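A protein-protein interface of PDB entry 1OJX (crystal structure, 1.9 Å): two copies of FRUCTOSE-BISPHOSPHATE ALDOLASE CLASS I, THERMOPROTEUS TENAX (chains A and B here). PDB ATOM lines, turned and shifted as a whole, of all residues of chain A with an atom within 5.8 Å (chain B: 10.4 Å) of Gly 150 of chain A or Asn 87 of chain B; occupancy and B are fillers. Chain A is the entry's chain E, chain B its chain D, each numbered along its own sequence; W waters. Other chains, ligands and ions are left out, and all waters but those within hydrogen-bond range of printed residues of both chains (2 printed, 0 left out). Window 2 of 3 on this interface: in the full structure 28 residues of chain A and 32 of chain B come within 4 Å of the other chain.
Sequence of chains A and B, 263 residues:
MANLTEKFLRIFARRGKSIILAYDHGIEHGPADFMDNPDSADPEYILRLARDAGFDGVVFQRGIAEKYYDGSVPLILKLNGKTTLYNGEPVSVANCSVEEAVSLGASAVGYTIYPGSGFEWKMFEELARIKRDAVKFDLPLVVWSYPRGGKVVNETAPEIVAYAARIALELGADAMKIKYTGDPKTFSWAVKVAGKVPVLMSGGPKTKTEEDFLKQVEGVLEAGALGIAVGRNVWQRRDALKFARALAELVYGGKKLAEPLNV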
ATOM      1  N   GLU A  89       6.608  10.242 -30.097  1.00  0.00           N
ATOM      2  CA  GLU A  89       5.946   9.698 -28.906  1.00  0.00           C
ATOM      3  C   GLU A  89       7.041   9.466 -27.841  1.00  0.00           C
ATOM      4  O   GLU A  89       8.110   8.980 -28.193  1.00  0.00           O
ATOM      5  CB  GLU A  89       5.242   8.368 -29.229  1.00  0.00           C
ATOM      6  CG  GLU A  89       3.834   8.469 -29.842  1.00  0.00           C
ATOM      7  CD  GLU A  89       2.827   9.274 -29.028  1.00  0.00           C
ATOM      8  OE1 GLU A  89       2.531   8.977 -27.845  1.00  0.00           O
ATOM      9  OE2 GLU A  89       2.277  10.234 -29.606  1.00  0.00           O
ATOM     10  N   GLY A 116       1.251   5.400 -21.154  1.00  0.00           N
ATOM     11  CA  GLY A 116       0.401   6.111 -22.087  1.00  0.00           C
ATOM     12  C   GLY A 116       1.033   6.376 -23.442  1.00  0.00           C
ATOM     13  O   GLY A 116       0.339   6.518 -24.439  1.00  0.00           O
ATOM     14  N   SER A 117       2.359   6.432 -23.497  1.00  0.00           N
ATOM     15  CA  SER A 117       3.060   6.708 -24.761  1.00  0.00           C
ATOM     16  C   SER A 117       2.770   5.616 -25.814  1.00  0.00           C
ATOM     17  O   SER A 117       2.605   4.440 -25.477  1.00  0.00           O
ATOM     18  CB  SER A 117       4.571   6.795 -24.509  1.00  0.00           C
ATOM     19  OG  SER A 117       5.273   7.025 -25.708  1.00  0.00           O
ATOM     20  N   GLY A 118       2.709   6.001 -27.081  1.00  0.00           N
ATOM     21  CA  GLY A 118       2.659   5.024 -28.168  1.00  0.00           C
ATOM     22  C   GLY A 118       3.795   4.000 -28.107  1.00  0.00           C
ATOM     23  O   GLY A 118       3.694   2.914 -28.690  1.00  0.00           O
ATOM     24  N   ARG A 148       2.728  10.203 -19.924  1.00  0.00           N
ATOM     25  CA  ARG A 148       2.916  11.197 -20.974  1.00  0.00           C
ATOM     26  C   ARG A 148       2.634  10.559 -22.332  1.00  0.00           C
ATOM     27  O   ARG A 148       3.090   9.456 -22.616  1.00  0.00           O
ATOM     28  CB  ARG A 148       4.349  11.710 -20.967  1.00  0.00           C
ATOM     29  CG  ARG A 148       4.564  12.999 -21.764  1.00  0.00           C
ATOM     30  CD  ARG A 148       5.932  13.634 -21.537  1.00  0.00           C
ATOM     31  NE  ARG A 148       6.055  14.099 -20.156  1.00  0.00           N
ATOM     32  CZ  ARG A 148       7.195  14.213 -19.494  1.00  0.00           C
ATOM     33  NH1 ARG A 148       8.352  13.908 -20.069  1.00  0.00           N
ATOM     34  NH2 ARG A 148       7.179  14.620 -18.239  1.00  0.00           N
ATOM     35  N   GLY A 149       1.903  11.270 -23.175  1.00  0.00           N
ATOM     36  CA  GLY A 149       1.486  10.743 -24.459  1.00  0.00           C
ATOM     37  C   GLY A 149       0.118  10.116 -24.305  1.00  0.00           C
ATOM     38  O   GLY A 149      -0.480  10.130 -23.207  1.00  0.00           O
ATOM     39  N   GLY A 150      -0.386   9.559 -25.402  1.00  0.00           N
ATOM     40  CA  GLY A 150      -1.691   8.924 -25.403  1.00  0.00           C
ATOM     41  C   GLY A 150      -2.794   9.851 -24.907  1.00  0.00           C
ATOM     42  O   GLY A 150      -2.932  10.974 -25.369  1.00  0.00           O
ATOM     43  N   LYS A 151      -3.556   9.374 -23.930  1.00  0.00           N
ATOM     44  CA  LYS A 151      -4.680  10.113 -23.368  1.00  0.00           C
ATOM     45  C   LYS A 151      -4.306  11.146 -22.299  1.00  0.00           C
ATOM     46  O   LYS A 151      -5.198  11.825 -21.773  1.00  0.00           O
ATOM     47  CB  LYS A 151      -5.672   9.129 -22.728  1.00  0.00           C
ATOM     48  CG  LYS A 151      -6.292   8.100 -23.672  1.00  0.00           C
ATOM     49  CD  LYS A 151      -7.298   7.220 -22.887  1.00  0.00           C
ATOM     50  CE  LYS A 151      -7.919   6.100 -23.755  1.00  0.00           C
ATOM     51  NZ  LYS A 151      -6.936   5.171 -24.357  1.00  0.00           N
ATOM     52  N   VAL A 152      -3.025  11.259 -21.938  1.00  0.00           N
ATOM     53  CA  VAL A 152      -2.627  12.130 -20.830  1.00  0.00           C
ATOM     54  C   VAL A 152      -2.672  13.599 -21.264  1.00  0.00           C
ATOM     55  O   VAL A 152      -1.973  13.977 -22.197  1.00  0.00           O
ATOM     56  CB  VAL A 152      -1.191  11.791 -20.306  1.00  0.00           C
ATOM     57  CG1 VAL A 152      -0.784  12.756 -19.219  1.00  0.00           C
ATOM     58  CG2 VAL A 152      -1.114  10.340 -19.779  1.00  0.00           C
ATOM     59  N   LYS B  82      -0.520  -3.839 -20.018  1.00  0.00           N
ATOM     60  CA  LYS B  82      -0.578  -2.514 -20.635  1.00  0.00           C
ATOM     61  C   LYS B  82      -1.490  -1.556 -19.824  1.00  0.00           C
ATOM     62  O   LYS B  82      -2.129  -1.987 -18.880  1.00  0.00           O
ATOM     63  CB  LYS B  82      -1.071  -2.643 -22.076  1.00  0.00           C
ATOM     64  CG  LYS B  82      -2.538  -3.037 -22.235  1.00  0.00           C
ATOM     65  CD  LYS B  82      -3.036  -2.651 -23.638  1.00  0.00           C
ATOM     66  CE  LYS B  82      -4.481  -2.167 -23.665  1.00  0.00           C
ATOM     67  NZ  LYS B  82      -4.864  -0.947 -22.892  1.00  0.00           N
ATOM     68  N   THR B  83      -1.530  -0.266 -20.180  1.00  0.00           N
ATOM     69  CA  THR B  83      -2.402   0.703 -19.499  1.00  0.00           C
ATOM     70  C   THR B  83      -3.540   1.155 -20.393  1.00  0.00           C
ATOM     71  O   THR B  83      -3.474   1.038 -21.621  1.00  0.00           O
ATOM     72  CB  THR B  83      -1.620   1.966 -19.002  1.00  0.00           C
ATOM     73  OG1 THR B  83      -1.239   2.791 -20.111  1.00  0.00           O
ATOM     74  CG2 THR B  83      -0.299   1.599 -18.317  1.00  0.00           C
ATOM     75  N   THR B  84      -4.586   1.705 -19.784  1.00  0.00           N
ATOM     76  CA  THR B  84      -5.654   2.340 -20.554  1.00  0.00           C
ATOM     77  C   THR B  84      -5.306   3.757 -21.003  1.00  0.00           C
ATOM     78  O   THR B  84      -6.078   4.372 -21.738  1.00  0.00           O
ATOM     79  CB  THR B  84      -6.984   2.413 -19.770  1.00  0.00           C
ATOM     80  OG1 THR B  84      -6.787   3.102 -18.531  1.00  0.00           O
ATOM     81  CG2 THR B  84      -7.451   1.055 -19.380  1.00  0.00           C
ATOM     82  N   LEU B  85      -4.166   4.284 -20.566  1.00  0.00           N
ATOM     83  CA  LEU B  85      -3.701   5.594 -21.037  1.00  0.00           C
ATOM     84  C   LEU B  85      -3.215   5.489 -22.496  1.00  0.00           C
ATOM     85  O   LEU B  85      -3.240   6.445 -23.253  1.00  0.00           O
ATOM     86  CB  LEU B  85      -2.592   6.114 -20.113  1.00  0.00           C
ATOM     87  CG  LEU B  85      -2.961   6.359 -18.644  1.00  0.00           C
ATOM     88  CD1 LEU B  85      -1.750   6.700 -17.808  1.00  0.00           C
ATOM     89  CD2 LEU B  85      -4.002   7.461 -18.516  1.00  0.00           C
ATOM     90  N   TYR B  86      -2.784   4.300 -22.876  1.00  0.00           N
ATOM     91  CA  TYR B  86      -2.215   4.040 -24.196  1.00  0.00           C
ATOM     92  C   TYR B  86      -3.325   4.142 -25.242  1.00  0.00           C
ATOM     93  O   TYR B  86      -4.433   3.683 -24.994  1.00  0.00           O
ATOM     94  CB  TYR B  86      -1.593   2.636 -24.181  1.00  0.00           C
ATOM     95  CG  TYR B  86      -1.160   2.076 -25.513  1.00  0.00           C
ATOM     96  CD1 TYR B  86       0.026   2.480 -26.105  1.00  0.00           C
ATOM     97  CD2 TYR B  86      -1.935   1.118 -26.171  1.00  0.00           C
ATOM     98  CE1 TYR B  86       0.444   1.955 -27.347  1.00  0.00           C
ATOM     99  CE2 TYR B  86      -1.536   0.585 -27.397  1.00  0.00           C
ATOM    100  CZ  TYR B  86      -0.336   1.006 -27.978  1.00  0.00           C
ATOM    101  OH  TYR B  86       0.042   0.493 -29.204  1.00  0.00           O
ATOM    102  N   ASN B  87      -3.016   4.757 -26.380  1.00  0.00           N
ATOM    103  CA  ASN B  87      -3.944   4.949 -27.497  1.00  0.00           C
ATOM    104  C   ASN B  87      -3.658   4.163 -28.782  1.00  0.00           C
ATOM    105  O   ASN B  87      -4.505   4.140 -29.674  1.00  0.00           O
ATOM    106  CB  ASN B  87      -3.949   6.434 -27.911  1.00  0.00           C
ATOM    107  CG  ASN B  87      -5.066   7.216 -27.290  1.00  0.00           C
ATOM    108  OD1 ASN B  87      -5.004   8.447 -27.232  1.00  0.00           O
ATOM    109  ND2 ASN B  87      -6.102   6.529 -26.844  1.00  0.00           N
ATOM    110  N   GLY B  88      -2.486   3.559 -28.924  1.00  0.00           N
ATOM    111  CA  GLY B  88      -2.154   2.858 -30.168  1.00  0.00           C
ATOM    112  C   GLY B  88      -2.941   1.573 -30.447  1.00  0.00           C
ATOM    113  O   GLY B  88      -3.953   1.277 -29.792  1.00  0.00           O
ATOM    114  N   GLU B  89      -2.475   0.806 -31.432  1.00  0.00           N
ATOM    115  CA  GLU B  89      -2.997  -0.537 -31.699  1.00  0.00           C
ATOM    116  C   GLU B  89      -2.751  -1.369 -30.470  1.00  0.00           C
ATOM    117  O   GLU B  89      -1.641  -1.333 -29.967  1.00  0.00           O
ATOM    118  CB  GLU B  89      -2.234  -1.218 -32.840  1.00  0.00           C
ATOM    119  CG  GLU B  89      -2.543  -0.679 -34.220  1.00  0.00           C
ATOM    120  CD  GLU B  89      -4.009  -0.745 -34.504  1.00  0.00           C
ATOM    121  OE1 GLU B  89      -4.614  -1.827 -34.323  1.00  0.00           O
ATOM    122  OE2 GLU B  89      -4.566   0.300 -34.871  1.00  0.00           O
ATOM    123  N   PRO B  90      -3.744  -2.128 -30.015  1.00  0.00           N
ATOM    124  CA  PRO B  90      -3.615  -2.937 -28.790  1.00  0.00           C
ATOM    125  C   PRO B  90      -2.362  -3.823 -28.745  1.00  0.00           C
ATOM    126  O   PRO B  90      -2.159  -4.640 -29.644  1.00  0.00           O
ATOM    127  CB  PRO B  90      -4.886  -3.805 -28.789  1.00  0.00           C
ATOM    128  CG  PRO B  90      -5.879  -3.068 -29.665  1.00  0.00           C
ATOM    129  CD  PRO B  90      -5.089  -2.232 -30.616  1.00  0.00           C
ATOM    130  N   VAL B  91      -1.555  -3.662 -27.697  1.00  0.00           N
ATOM    131  CA  VAL B  91      -0.341  -4.450 -27.519  1.00  0.00           C
ATOM    132  C   VAL B  91       0.030  -4.479 -26.041  1.00  0.00           C
ATOM    133  O   VAL B  91      -0.144  -3.488 -25.316  1.00  0.00           O
ATOM    134  CB  VAL B  91       0.845  -3.913 -28.374  1.00  0.00           C
ATOM    135  CG1 VAL B  91       1.303  -2.538 -27.920  1.00  0.00           C
ATOM    136  CG2 VAL B  91       2.028  -4.902 -28.371  1.00  0.00           C
ATOM    137  N   SER B 117      -5.505  -7.161 -33.722  1.00  0.00           N
ATOM    138  CA  SER B 117      -4.713  -5.935 -33.576  1.00  0.00           C
ATOM    139  C   SER B 117      -3.691  -5.798 -34.712  1.00  0.00           C
ATOM    140  O   SER B 117      -3.176  -6.785 -35.219  1.00  0.00           O
ATOM    141  CB  SER B 117      -3.986  -5.928 -32.214  1.00  0.00           C
ATOM    142  OG  SER B 117      -3.023  -4.891 -32.134  1.00  0.00           O
ATOM    143  N   GLY B 118      -3.384  -4.565 -35.082  1.00  0.00           N
ATOM    144  CA  GLY B 118      -2.247  -4.278 -35.947  1.00  0.00           C
ATOM    145  C   GLY B 118      -0.939  -4.860 -35.446  1.00  0.00           C
ATOM    146  O   GLY B 118      -0.048  -5.115 -36.242  1.00  0.00           O
ATOM    147  N   PHE B 119      -0.840  -5.084 -34.132  1.00  0.00           N
ATOM    148  CA  PHE B 119       0.308  -5.735 -33.488  1.00  0.00           C
ATOM    149  C   PHE B 119       0.056  -7.207 -33.107  1.00  0.00           C
ATOM    150  O   PHE B 119       0.769  -7.746 -32.251  1.00  0.00           O
ATOM    151  CB  PHE B 119       0.654  -5.005 -32.180  1.00  0.00           C
ATOM    152  CG  PHE B 119       1.494  -3.768 -32.349  1.00  0.00           C
ATOM    153  CD1 PHE B 119       1.002  -2.531 -31.964  1.00  0.00           C
ATOM    154  CD2 PHE B 119       2.802  -3.853 -32.819  1.00  0.00           C
ATOM    155  CE1 PHE B 119       1.777  -1.387 -32.085  1.00  0.00           C
ATOM    156  CE2 PHE B 119       3.593  -2.713 -32.937  1.00  0.00           C
ATOM    157  CZ  PHE B 119       3.073  -1.474 -32.574  1.00  0.00           C
ATOM    158  N   ARG B 148      -9.360  -7.560 -30.372  1.00  0.00           N
ATOM    159  CA  ARG B 148      -9.459  -6.110 -30.254  1.00  0.00           C
ATOM    160  C   ARG B 148      -8.628  -5.496 -31.354  1.00  0.00           C
ATOM    161  O   ARG B 148      -7.526  -5.969 -31.650  1.00  0.00           O
ATOM    162  CB  ARG B 148      -8.958  -5.642 -28.878  1.00  0.00           C
ATOM    163  CG  ARG B 148      -9.365  -4.231 -28.487  1.00  0.00           C
ATOM    164  CD  ARG B 148      -9.063  -3.895 -27.015  1.00  0.00           C
ATOM    165  NE  ARG B 148      -9.906  -4.681 -26.116  1.00  0.00           N
ATOM    166  CZ  ARG B 148      -9.626  -4.984 -24.855  1.00  0.00           C
ATOM    167  NH1 ARG B 148      -8.507  -4.578 -24.266  1.00  0.00           N
ATOM    168  NH2 ARG B 148     -10.494  -5.698 -24.163  1.00  0.00           N
ATOM    169  N   GLY B 149      -9.165  -4.439 -31.957  1.00  0.00           N
ATOM    170  CA  GLY B 149      -8.536  -3.771 -33.074  1.00  0.00           C
ATOM    171  C   GLY B 149      -8.909  -4.477 -34.357  1.00  0.00           C
ATOM    172  O   GLY B 149      -9.742  -5.390 -34.366  1.00  0.00           O
HETATM  173  O   HOH W   1      -0.601   5.982 -26.956  1.00  0.00           O
HETATM  174  O   HOH W   2       2.174   1.961 -30.524  1.00  0.00           O
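Water W2 lies within hydrogen-bond range of O of Gly 118 of chain A and OH of Tyr 86 of chain B. Water W1 lies within hydrogen-bond range of the backbone carbonyl oxygen of Gly 116 of chain A (2.7 Å), the backbone NH of Asn 87 of chain B (2.8 Å) and the backbone NH of Gly 118 of chain A (3.3 Å).
Among the printed residues, merely in contact across the chains: Ser 117 of chain A with Tyr 86 of chain B (3.3 Å), Gly 150 of chain A with Asn 87 of chain B (3.5 Å), Gly 116 of chain A with Tyr 86 of chain B (3.6 Å), Gly 116 of chain A with Leu 85 of chain B (3.6 Å), Gly 150 of chain A with Leu 85 of chain B (3.6 Å), Gly 118 of chain A with Tyr 86 of chain B (3.6 Å) and Gly 116 of chain A with Thr 83 of chain B (3.8 Å).
Hydrophobic or aromatic side chains of chain B within 4 Å of the printed part of chain A: Leu 85 and Tyr 86.
N of Leu 85 of chain B lies close to OG1 of Thr 83 of chain B (3.3 Å). OH of Tyr 86 of chain B lies within hydrogen-bond range of O of Glu 89 of chain B. The backbone NH (N) of Gly 118 of chain A is in hydrogen-bond range of the side-chain carboxylate (OE1) of Glu 89 of chain A (3.1 Å). The backbone NH (N) of Gly 150 of chain A lies within hydrogen-bond range of the backbone carbonyl oxygen (O) of Gly 116 of chain A, at 3.3 Å. The backbone carbonyl oxygen (O) of Arg 148 of chain A sits at hydrogen-bond distance from the backbone NH (N) of Ser 117 of chain A (3.2 Å).
The backbone carbonyl oxygen (O) of Thr 84 of chain B is in hydrogen-bond range of the side-chain amino group (NZ) of Lys 151 of chain A, 2.9 Å away. The backbone NH of Lys 151 of chain A lies within hydrogen-bond range of the backbone carbonyl oxygen of Leu 85 of chain B, 3.0 Å away. O of Tyr 86 of chain B sits at hydrogen-bond distance from NZ of Lys 151 of chain A, 3.0 Å away. NZ of Lys 151 of chain A sits close to ND2 of Asn 87 of chain B, at 3.0 Å.
Of chain B, only Tyr 86 comes within 4 Å of Ser 117 of chain A. No residue of chain B comes within 4 Å of Gly 149 of chain A. Of chain B, only Leu 85 (3.6 Å) and Asn 87 (3.5 Å) come within 4 Å of Gly 150 of chain A. Lys 151 of chain A touches four residues of chain B. Val 152 of chain A touches none of the printed residues of chain B. Of the printed residues of chain A, Thr 83 of chain B touches Gly 116. Of the printed residues of chain A, Leu 85 of chain B touches Gly 116, Gly 150 and Lys 151. Of chain A, only Gly 150 and Lys 151 come within 4 Å of Asn 87 of chain B. Arg 148 of chain B touches none of the printed residues of chain A. The nearest residue of chain B that does not touch Gly 150 of chain A is Tyr 86 of chain B (5.1 Å). The nearest residue of chain A that does not touch Asn 87 of chain B is Gly 116 of chain A (4.3 Å). The nearest printed residue of chain A that does not touch Thr 84 of chain B is Gly 116 of chain A (6.3 Å).
Positions printed for both chains: 89, 117, 118, 148 and 149. Of the 11 pairs that touch across the chains among the printed residues, none has its exchanged pair printed and touching as well.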
